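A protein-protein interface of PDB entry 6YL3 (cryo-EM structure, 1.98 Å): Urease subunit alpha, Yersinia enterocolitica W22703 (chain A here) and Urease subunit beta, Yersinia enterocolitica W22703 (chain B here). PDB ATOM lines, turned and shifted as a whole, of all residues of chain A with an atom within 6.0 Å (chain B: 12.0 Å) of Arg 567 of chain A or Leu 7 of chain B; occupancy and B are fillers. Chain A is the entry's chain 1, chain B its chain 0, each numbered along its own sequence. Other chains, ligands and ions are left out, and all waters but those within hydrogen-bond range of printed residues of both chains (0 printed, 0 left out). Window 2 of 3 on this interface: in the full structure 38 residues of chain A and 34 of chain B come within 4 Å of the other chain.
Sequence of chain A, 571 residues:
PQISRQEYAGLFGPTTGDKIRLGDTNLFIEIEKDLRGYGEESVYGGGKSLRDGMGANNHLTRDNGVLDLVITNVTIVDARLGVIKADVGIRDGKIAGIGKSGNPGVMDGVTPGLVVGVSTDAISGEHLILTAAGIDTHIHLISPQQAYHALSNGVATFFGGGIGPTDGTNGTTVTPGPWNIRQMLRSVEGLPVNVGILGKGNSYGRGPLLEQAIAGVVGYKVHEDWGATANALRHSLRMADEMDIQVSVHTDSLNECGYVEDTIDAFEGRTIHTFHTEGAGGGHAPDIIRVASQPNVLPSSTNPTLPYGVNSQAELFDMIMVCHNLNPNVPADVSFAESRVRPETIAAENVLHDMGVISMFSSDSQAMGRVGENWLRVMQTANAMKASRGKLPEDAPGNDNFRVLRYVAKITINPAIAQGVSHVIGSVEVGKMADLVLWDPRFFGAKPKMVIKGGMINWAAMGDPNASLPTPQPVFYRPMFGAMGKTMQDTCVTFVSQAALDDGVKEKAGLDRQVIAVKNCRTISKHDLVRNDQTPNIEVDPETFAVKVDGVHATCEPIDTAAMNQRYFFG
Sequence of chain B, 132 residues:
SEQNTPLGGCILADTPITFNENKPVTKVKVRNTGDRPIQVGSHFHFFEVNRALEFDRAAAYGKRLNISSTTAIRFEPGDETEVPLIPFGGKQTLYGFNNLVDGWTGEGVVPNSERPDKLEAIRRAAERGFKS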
ATOM      1  N   ARG A  21     -32.454   3.379  -8.662  1.00  0.00           N
ATOM      2  CA  ARG A  21     -31.382   2.573  -9.141  1.00  0.00           C
ATOM      3  C   ARG A  21     -30.911   3.098 -10.496  1.00  0.00           C
ATOM      4  O   ARG A  21     -31.703   3.377 -11.371  1.00  0.00           O
ATOM      5  CB  ARG A  21     -31.763   1.129  -9.248  1.00  0.00           C
ATOM      6  CG  ARG A  21     -30.708   0.156  -9.417  1.00  0.00           C
ATOM      7  CD  ARG A  21     -30.932  -1.156  -9.460  1.00  0.00           C
ATOM      8  NE  ARG A  21     -29.830  -2.019  -9.640  1.00  0.00           N
ATOM      9  CZ  ARG A  21     -29.799  -3.263  -9.950  1.00  0.00           C
ATOM     10  NH1 ARG A  21     -30.826  -3.949 -10.165  1.00  0.00           N
ATOM     11  NH2 ARG A  21     -28.677  -3.834 -10.115  1.00  0.00           N
ATOM     12  N   GLY A  23     -29.103   2.080 -13.342  1.00  0.00           N
ATOM     13  CA  GLY A  23     -28.846   0.975 -14.148  1.00  0.00           C
ATOM     14  C   GLY A  23     -28.875  -0.309 -13.495  1.00  0.00           C
ATOM     15  O   GLY A  23     -29.698  -0.585 -12.650  1.00  0.00           O
ATOM     16  N   ASP A  24     -27.898  -1.080 -13.875  1.00  0.00           N
ATOM     17  CA  ASP A  24     -27.512  -2.296 -13.271  1.00  0.00           C
ATOM     18  C   ASP A  24     -26.450  -2.149 -12.240  1.00  0.00           C
ATOM     19  O   ASP A  24     -25.878  -3.128 -11.849  1.00  0.00           O
ATOM     20  CB  ASP A  24     -27.140  -3.264 -14.325  1.00  0.00           C
ATOM     21  CG  ASP A  24     -25.724  -3.128 -14.912  1.00  0.00           C
ATOM     22  OD1 ASP A  24     -25.067  -2.092 -14.821  1.00  0.00           O
ATOM     23  OD2 ASP A  24     -25.354  -4.113 -15.533  1.00  0.00           O
ATOM     24  N   PRO A 441     -33.390   5.921 -16.488  1.00  0.00           N
ATOM     25  CA  PRO A 441     -32.641   5.269 -15.422  1.00  0.00           C
ATOM     26  C   PRO A 441     -32.143   3.954 -15.662  1.00  0.00           C
ATOM     27  O   PRO A 441     -31.075   3.667 -15.226  1.00  0.00           O
ATOM     28  CB  PRO A 441     -33.602   5.316 -14.242  1.00  0.00           C
ATOM     29  CG  PRO A 441     -34.524   6.237 -14.547  1.00  0.00           C
ATOM     30  CD  PRO A 441     -34.616   6.468 -15.908  1.00  0.00           C
ATOM     31  N   ARG A 442     -32.852   3.193 -16.374  1.00  0.00           N
ATOM     32  CA  ARG A 442     -32.470   1.913 -16.771  1.00  0.00           C
ATOM     33  C   ARG A 442     -31.116   1.844 -17.547  1.00  0.00           C
ATOM     34  O   ARG A 442     -30.490   0.822 -17.538  1.00  0.00           O
ATOM     35  CB  ARG A 442     -33.552   1.304 -17.576  1.00  0.00           C
ATOM     36  CG  ARG A 442     -34.992   1.065 -17.087  1.00  0.00           C
ATOM     37  CD  ARG A 442     -35.966   0.684 -18.028  1.00  0.00           C
ATOM     38  NE  ARG A 442     -36.258   1.434 -19.135  1.00  0.00           N
ATOM     39  CZ  ARG A 442     -36.785   0.975 -20.213  1.00  0.00           C
ATOM     40  NH1 ARG A 442     -36.984  -0.251 -20.418  1.00  0.00           N
ATOM     41  NH2 ARG A 442     -36.966   1.814 -21.119  1.00  0.00           N
ATOM     42  N   ALA A 562     -17.572  -5.384 -15.094  1.00  0.00           N
ATOM     43  CA  ALA A 562     -18.114  -4.072 -15.179  1.00  0.00           C
ATOM     44  C   ALA A 562     -19.638  -4.059 -15.387  1.00  0.00           C
ATOM     45  O   ALA A 562     -20.234  -4.925 -16.012  1.00  0.00           O
ATOM     46  CB  ALA A 562     -17.404  -3.245 -16.225  1.00  0.00           C
ATOM     47  N   MET A 564     -23.083  -1.744 -16.671  1.00  0.00           N
ATOM     48  CA  MET A 564     -23.435  -0.860 -17.791  1.00  0.00           C
ATOM     49  C   MET A 564     -22.494  -1.286 -18.932  1.00  0.00           C
ATOM     50  O   MET A 564     -21.819  -0.475 -19.421  1.00  0.00           O
ATOM     51  CB  MET A 564     -23.239   0.632 -17.503  1.00  0.00           C
ATOM     52  CG  MET A 564     -23.921   1.131 -16.217  1.00  0.00           C
ATOM     53  SD  MET A 564     -25.702   0.806 -16.271  1.00  0.00           S
ATOM     54  CE  MET A 564     -26.127   1.315 -17.940  1.00  0.00           C
ATOM     55  N   ASN A 565     -22.294  -2.550 -19.153  1.00  0.00           N
ATOM     56  CA  ASN A 565     -21.168  -2.980 -20.007  1.00  0.00           C
ATOM     57  C   ASN A 565     -21.666  -3.966 -21.072  1.00  0.00           C
ATOM     58  O   ASN A 565     -22.330  -3.493 -21.921  1.00  0.00           O
ATOM     59  CB  ASN A 565     -19.912  -3.319 -19.201  1.00  0.00           C
ATOM     60  CG  ASN A 565     -18.803  -3.639 -20.168  1.00  0.00           C
ATOM     61  OD1 ASN A 565     -18.520  -2.841 -21.028  1.00  0.00           O
ATOM     62  ND2 ASN A 565     -18.311  -4.840 -20.101  1.00  0.00           N
ATOM     63  N   GLN A 566     -21.476  -5.269 -20.966  1.00  0.00           N
ATOM     64  CA  GLN A 566     -21.822  -6.279 -22.001  1.00  0.00           C
ATOM     65  C   GLN A 566     -23.360  -6.482 -22.105  1.00  0.00           C
ATOM     66  O   GLN A 566     -23.811  -6.897 -23.121  1.00  0.00           O
ATOM     67  CB  GLN A 566     -21.104  -7.576 -21.660  1.00  0.00           C
ATOM     68  CG  GLN A 566     -19.639  -7.627 -22.101  1.00  0.00           C
ATOM     69  CD  GLN A 566     -19.040  -9.014 -22.056  1.00  0.00           C
ATOM     70  OE1 GLN A 566     -19.538  -9.864 -21.360  1.00  0.00           O
ATOM     71  NE2 GLN A 566     -17.946  -9.240 -22.766  1.00  0.00           N
ATOM     72  N   ARG A 567     -24.144  -6.169 -21.093  1.00  0.00           N
ATOM     73  CA  ARG A 567     -25.603  -6.204 -21.081  1.00  0.00           C
ATOM     74  C   ARG A 567     -26.261  -5.273 -22.086  1.00  0.00           C
ATOM     75  O   ARG A 567     -27.282  -5.592 -22.638  1.00  0.00           O
ATOM     76  CB  ARG A 567     -26.048  -5.925 -19.641  1.00  0.00           C
ATOM     77  CG  ARG A 567     -27.235  -6.554 -19.189  1.00  0.00           C
ATOM     78  CD  ARG A 567     -27.657  -6.053 -17.950  1.00  0.00           C
ATOM     79  NE  ARG A 567     -26.666  -6.194 -16.889  1.00  0.00           N
ATOM     80  CZ  ARG A 567     -26.456  -7.291 -16.246  1.00  0.00           C
ATOM     81  NH1 ARG A 567     -27.124  -8.321 -16.471  1.00  0.00           N
ATOM     82  NH2 ARG A 567     -25.574  -7.373 -15.336  1.00  0.00           N
ATOM     83  N   TYR A 568     -25.759  -4.139 -22.226  1.00  0.00           N
ATOM     84  CA  TYR A 568     -26.170  -2.932 -22.923  1.00  0.00           C
ATOM     85  C   TYR A 568     -25.560  -2.707 -24.317  1.00  0.00           C
ATOM     86  O   TYR A 568     -26.170  -2.076 -25.121  1.00  0.00           O
ATOM     87  CB  TYR A 568     -25.918  -1.750 -22.080  1.00  0.00           C
ATOM     88  CG  TYR A 568     -26.655  -1.580 -20.761  1.00  0.00           C
ATOM     89  CD1 TYR A 568     -26.373  -2.303 -19.669  1.00  0.00           C
ATOM     90  CD2 TYR A 568     -27.701  -0.806 -20.658  1.00  0.00           C
ATOM     91  CE1 TYR A 568     -27.073  -2.149 -18.572  1.00  0.00           C
ATOM     92  CE2 TYR A 568     -28.376  -0.714 -19.619  1.00  0.00           C
ATOM     93  CZ  TYR A 568     -28.074  -1.353 -18.530  1.00  0.00           C
ATOM     94  OH  TYR A 568     -28.773  -1.341 -17.388  1.00  0.00           O
ATOM     95  N   PHE A 569     -24.424  -3.249 -24.618  1.00  0.00           N
ATOM     96  CA  PHE A 569     -23.633  -2.908 -25.775  1.00  0.00           C
ATOM     97  C   PHE A 569     -23.318  -4.139 -26.639  1.00  0.00           C
ATOM     98  O   PHE A 569     -22.957  -5.178 -26.137  1.00  0.00           O
ATOM     99  CB  PHE A 569     -22.422  -2.089 -25.454  1.00  0.00           C
ATOM    100  CG  PHE A 569     -22.633  -0.730 -24.928  1.00  0.00           C
ATOM    101  CD1 PHE A 569     -22.775   0.344 -25.693  1.00  0.00           C
ATOM    102  CD2 PHE A 569     -22.576  -0.494 -23.678  1.00  0.00           C
ATOM    103  CE1 PHE A 569     -22.859   1.482 -25.150  1.00  0.00           C
ATOM    104  CE2 PHE A 569     -22.664   0.652 -23.229  1.00  0.00           C
ATOM    105  CZ  PHE A 569     -22.826   1.598 -23.925  1.00  0.00           C
ATOM    106  N   SER B   1     -36.169  -3.652  -1.482  1.00  0.00           N
ATOM    107  CA  SER B   1     -35.053  -3.582  -0.504  1.00  0.00           C
ATOM    108  C   SER B   1     -33.874  -2.781  -1.062  1.00  0.00           C
ATOM    109  O   SER B   1     -33.527  -1.781  -0.409  1.00  0.00           O
ATOM    110  CB  SER B   1     -34.581  -4.960  -0.114  1.00  0.00           C
ATOM    111  OG  SER B   1     -34.236  -5.722  -1.269  1.00  0.00           O
ATOM    112  N   GLU B   2     -33.395  -3.209  -2.243  1.00  0.00           N
ATOM    113  CA  GLU B   2     -32.205  -2.771  -3.040  1.00  0.00           C
ATOM    114  C   GLU B   2     -31.688  -3.963  -3.832  1.00  0.00           C
ATOM    115  O   GLU B   2     -31.532  -3.816  -5.059  1.00  0.00           O
ATOM    116  CB  GLU B   2     -31.004  -2.230  -2.275  1.00  0.00           C
ATOM    117  CG  GLU B   2     -30.980  -0.732  -2.136  1.00  0.00           C
ATOM    118  CD  GLU B   2     -29.625  -0.224  -1.681  1.00  0.00           C
ATOM    119  OE1 GLU B   2     -28.628  -0.967  -1.869  1.00  0.00           O
ATOM    120  OE2 GLU B   2     -29.548   0.879  -1.101  1.00  0.00           O
ATOM    121  N   GLN B   3     -31.627  -5.131  -3.176  1.00  0.00           N
ATOM    122  CA  GLN B   3     -31.186  -6.448  -3.710  1.00  0.00           C
ATOM    123  C   GLN B   3     -32.186  -6.987  -4.742  1.00  0.00           C
ATOM    124  O   GLN B   3     -31.804  -7.892  -5.482  1.00  0.00           O
ATOM    125  CB  GLN B   3     -31.153  -7.501  -2.593  1.00  0.00           C
ATOM    126  CG  GLN B   3     -30.385  -7.081  -1.345  1.00  0.00           C
ATOM    127  CD  GLN B   3     -31.240  -6.388  -0.309  1.00  0.00           C
ATOM    128  OE1 GLN B   3     -32.128  -6.991   0.300  1.00  0.00           O
ATOM    129  NE2 GLN B   3     -30.948  -5.117  -0.072  1.00  0.00           N
ATOM    130  N   ASN B   4     -33.430  -6.498  -4.719  1.00  0.00           N
ATOM    131  CA  ASN B   4     -34.570  -6.926  -5.517  1.00  0.00           C
ATOM    132  C   ASN B   4     -35.079  -5.970  -6.598  1.00  0.00           C
ATOM    133  O   ASN B   4     -35.947  -6.363  -7.358  1.00  0.00           O
ATOM    134  CB  ASN B   4     -35.726  -7.129  -4.556  1.00  0.00           C
ATOM    135  CG  ASN B   4     -36.171  -5.837  -3.926  1.00  0.00           C
ATOM    136  OD1 ASN B   4     -35.316  -4.989  -3.583  1.00  0.00           O
ATOM    137  ND2 ASN B   4     -37.461  -5.634  -3.772  1.00  0.00           N
ATOM    138  N   THR B   5     -34.699  -4.720  -6.583  1.00  0.00           N
ATOM    139  CA  THR B   5     -35.122  -3.742  -7.556  1.00  0.00           C
ATOM    140  C   THR B   5     -34.655  -4.086  -8.958  1.00  0.00           C
ATOM    141  O   THR B   5     -33.495  -4.380  -9.142  1.00  0.00           O
ATOM    142  CB  THR B   5     -34.566  -2.452  -7.092  1.00  0.00           C
ATOM    143  OG1 THR B   5     -34.962  -2.181  -5.782  1.00  0.00           O
ATOM    144  CG2 THR B   5     -34.839  -1.361  -7.885  1.00  0.00           C
ATOM    145  N   PRO B   6     -35.518  -4.070  -9.958  1.00  0.00           N
ATOM    146  CA  PRO B   6     -35.051  -4.216 -11.349  1.00  0.00           C
ATOM    147  C   PRO B   6     -34.125  -3.083 -11.776  1.00  0.00           C
ATOM    148  O   PRO B   6     -34.110  -2.046 -11.140  1.00  0.00           O
ATOM    149  CB  PRO B   6     -36.361  -4.203 -12.119  1.00  0.00           C
ATOM    150  CG  PRO B   6     -37.229  -3.619 -11.279  1.00  0.00           C
ATOM    151  CD  PRO B   6     -36.951  -3.872  -9.973  1.00  0.00           C
ATOM    152  N   LEU B   7     -33.459  -3.295 -12.926  1.00  0.00           N
ATOM    153  CA  LEU B   7     -32.621  -2.276 -13.587  1.00  0.00           C
ATOM    154  C   LEU B   7     -33.508  -1.033 -13.727  1.00  0.00           C
ATOM    155  O   LEU B   7     -34.472  -1.133 -14.263  1.00  0.00           O
ATOM    156  CB  LEU B   7     -32.131  -2.687 -14.980  1.00  0.00           C
ATOM    157  CG  LEU B   7     -31.438  -4.034 -15.159  1.00  0.00           C
ATOM    158  CD1 LEU B   7     -30.617  -4.018 -16.441  1.00  0.00           C
ATOM    159  CD2 LEU B   7     -30.579  -4.414 -13.975  1.00  0.00           C
ATOM    160  N   GLY B   8     -33.085   0.121 -13.315  1.00  0.00           N
ATOM    161  CA  GLY B   8     -33.647   1.406 -13.282  1.00  0.00           C
ATOM    162  C   GLY B   8     -34.795   1.602 -12.358  1.00  0.00           C
ATOM    163  O   GLY B   8     -35.389   2.663 -12.391  1.00  0.00           O
ATOM    164  N   GLY B   9     -35.048   0.621 -11.519  1.00  0.00           N
ATOM    165  CA  GLY B   9     -36.166   0.613 -10.686  1.00  0.00           C
ATOM    166  C   GLY B   9     -36.063   1.559  -9.545  1.00  0.00           C
ATOM    167  O   GLY B   9     -35.036   2.080  -9.176  1.00  0.00           O
ATOM    168  N   CYS B  10     -37.214   1.778  -9.047  1.00  0.00           N
ATOM    169  CA  CYS B  10     -37.537   2.629  -7.944  1.00  0.00           C
ATOM    170  C   CYS B  10     -37.855   1.835  -6.679  1.00  0.00           C
ATOM    171  O   CYS B  10     -38.434   0.767  -6.720  1.00  0.00           O
ATOM    172  CB  CYS B  10     -38.644   3.567  -8.320  1.00  0.00           C
ATOM    173  SG  CYS B  10     -40.212   2.857  -8.318  1.00  0.00           S
ATOM    174  N   ILE B  11     -37.365   2.331  -5.584  1.00  0.00           N
ATOM    175  CA  ILE B  11     -37.743   1.944  -4.227  1.00  0.00           C
ATOM    176  C   ILE B  11     -38.548   3.078  -3.666  1.00  0.00           C
ATOM    177  O   ILE B  11     -38.007   4.130  -3.336  1.00  0.00           O
ATOM    178  CB  ILE B  11     -36.583   1.692  -3.259  1.00  0.00           C
ATOM    179  CG1 ILE B  11     -35.675   0.603  -3.714  1.00  0.00           C
ATOM    180  CG2 ILE B  11     -37.151   1.492  -1.789  1.00  0.00           C
ATOM    181  CD1 ILE B  11     -34.483   0.390  -2.844  1.00  0.00           C
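Of the 12 printed residues of chain A, 7 touch a printed residue of chain B. Hydrophobic or aromatic side chains of chain A within 4 Å of the printed part of chain B: Pro 441 and Tyr 568. Along chain A the printed residues that touch a printed residue of chain B span positions 21 to 568. Hydrophobic or aromatic side chains of chain B within 4 Å of the printed part of chain A: Leu 7. Among the printed residues, no Asp or Glu carboxylate lies within 4 Å of a Lys or Arg side-chain nitrogen of the other chain.
Gly 23 of chain A touches just these residues of chain B: Leu 7 and Gly 8. Arg 442 of chain A touches just these residues of chain B: Leu 7 and Gly 8. No residue of chain B comes within 4 Å of Met 564 of chain A. No residue of chain B comes within 4 Å of Gln 566 of chain A. Printed residues of chain A within 4 Å of Pro 6 of chain B: Arg 21. Of the printed residues of chain A, Leu 7 of chain B touches Arg 21, Gly 23, Asp 24, Arg 442, Arg 567 and Tyr 568. Of the printed residues of chain A, Gly 8 of chain B touches Arg 21, Gly 23, Pro 441 and Arg 442. Cys 10 of chain B touches none of the printed residues of chain A. The nearest residue of chain A that does not touch Leu 7 of chain B is Pro 441 of chain A (5.5 Å).
Among the printed residues, merely in contact across the chains: Arg 21 of chain A with Pro 6 of chain B (3.7 Å), Arg 21 of chain A with Leu 7 of chain B (3.8 Å), Arg 21 of chain A with Gly 8 of chain B (3.4 Å), Gly 23 of chain A with Leu 7 of chain B (3.5 Å), Gly 23 of chain A with Gly 8 of chain B (3.5 Å), Asp 24 of chain A with Leu 7 of chain B (3.6 Å), Pro 441 of chain A with Gly 8 of chain B (3.7 Å), Arg 442 of chain A with Leu 7 of chain B (3.6 Å), Arg 442 of chain A with Gly 8 of chain B (3.7 Å), Arg 567 of chain A with Leu 7 of chain B (3.9 Å) and Tyr 568 of chain A with Leu 7 of chain B (3.4 Å).
The guanidinium group of Arg 21 of chain A sits at hydrogen-bond distance from the backbone carbonyl oxygen of Gly 23 of chain A, 3.3 Å away. NH2 of Arg 21 of chain A is in hydrogen-bond range of O of Asp 24 of chain A. The backbone carbonyl oxygen of Pro 441 of chain A lies within hydrogen-bond range of the backbone NH of Gly 23 of chain A, 3.2 Å away. OD1 of Asp 24 of chain A is in hydrogen-bond range of N of Met 564 of chain A, 2.7 Å away. The side-chain carboxylate (OD2) of Asp 24 of chain A is in salt-bridge range of the guanidinium group (NE) of Arg 567 of chain A (2.8 Å). OH of Tyr 568 of chain A sits at hydrogen-bond distance from O of Arg 442 of chain A (2.8 Å).
O of Thr 5 of chain B lies within hydrogen-bond range of NH1 of Arg 21 of chain A (2.9 Å). N of Arg 21 of chain A lies within hydrogen-bond range of O of Gly 9 of chain B, 2.9 Å away.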
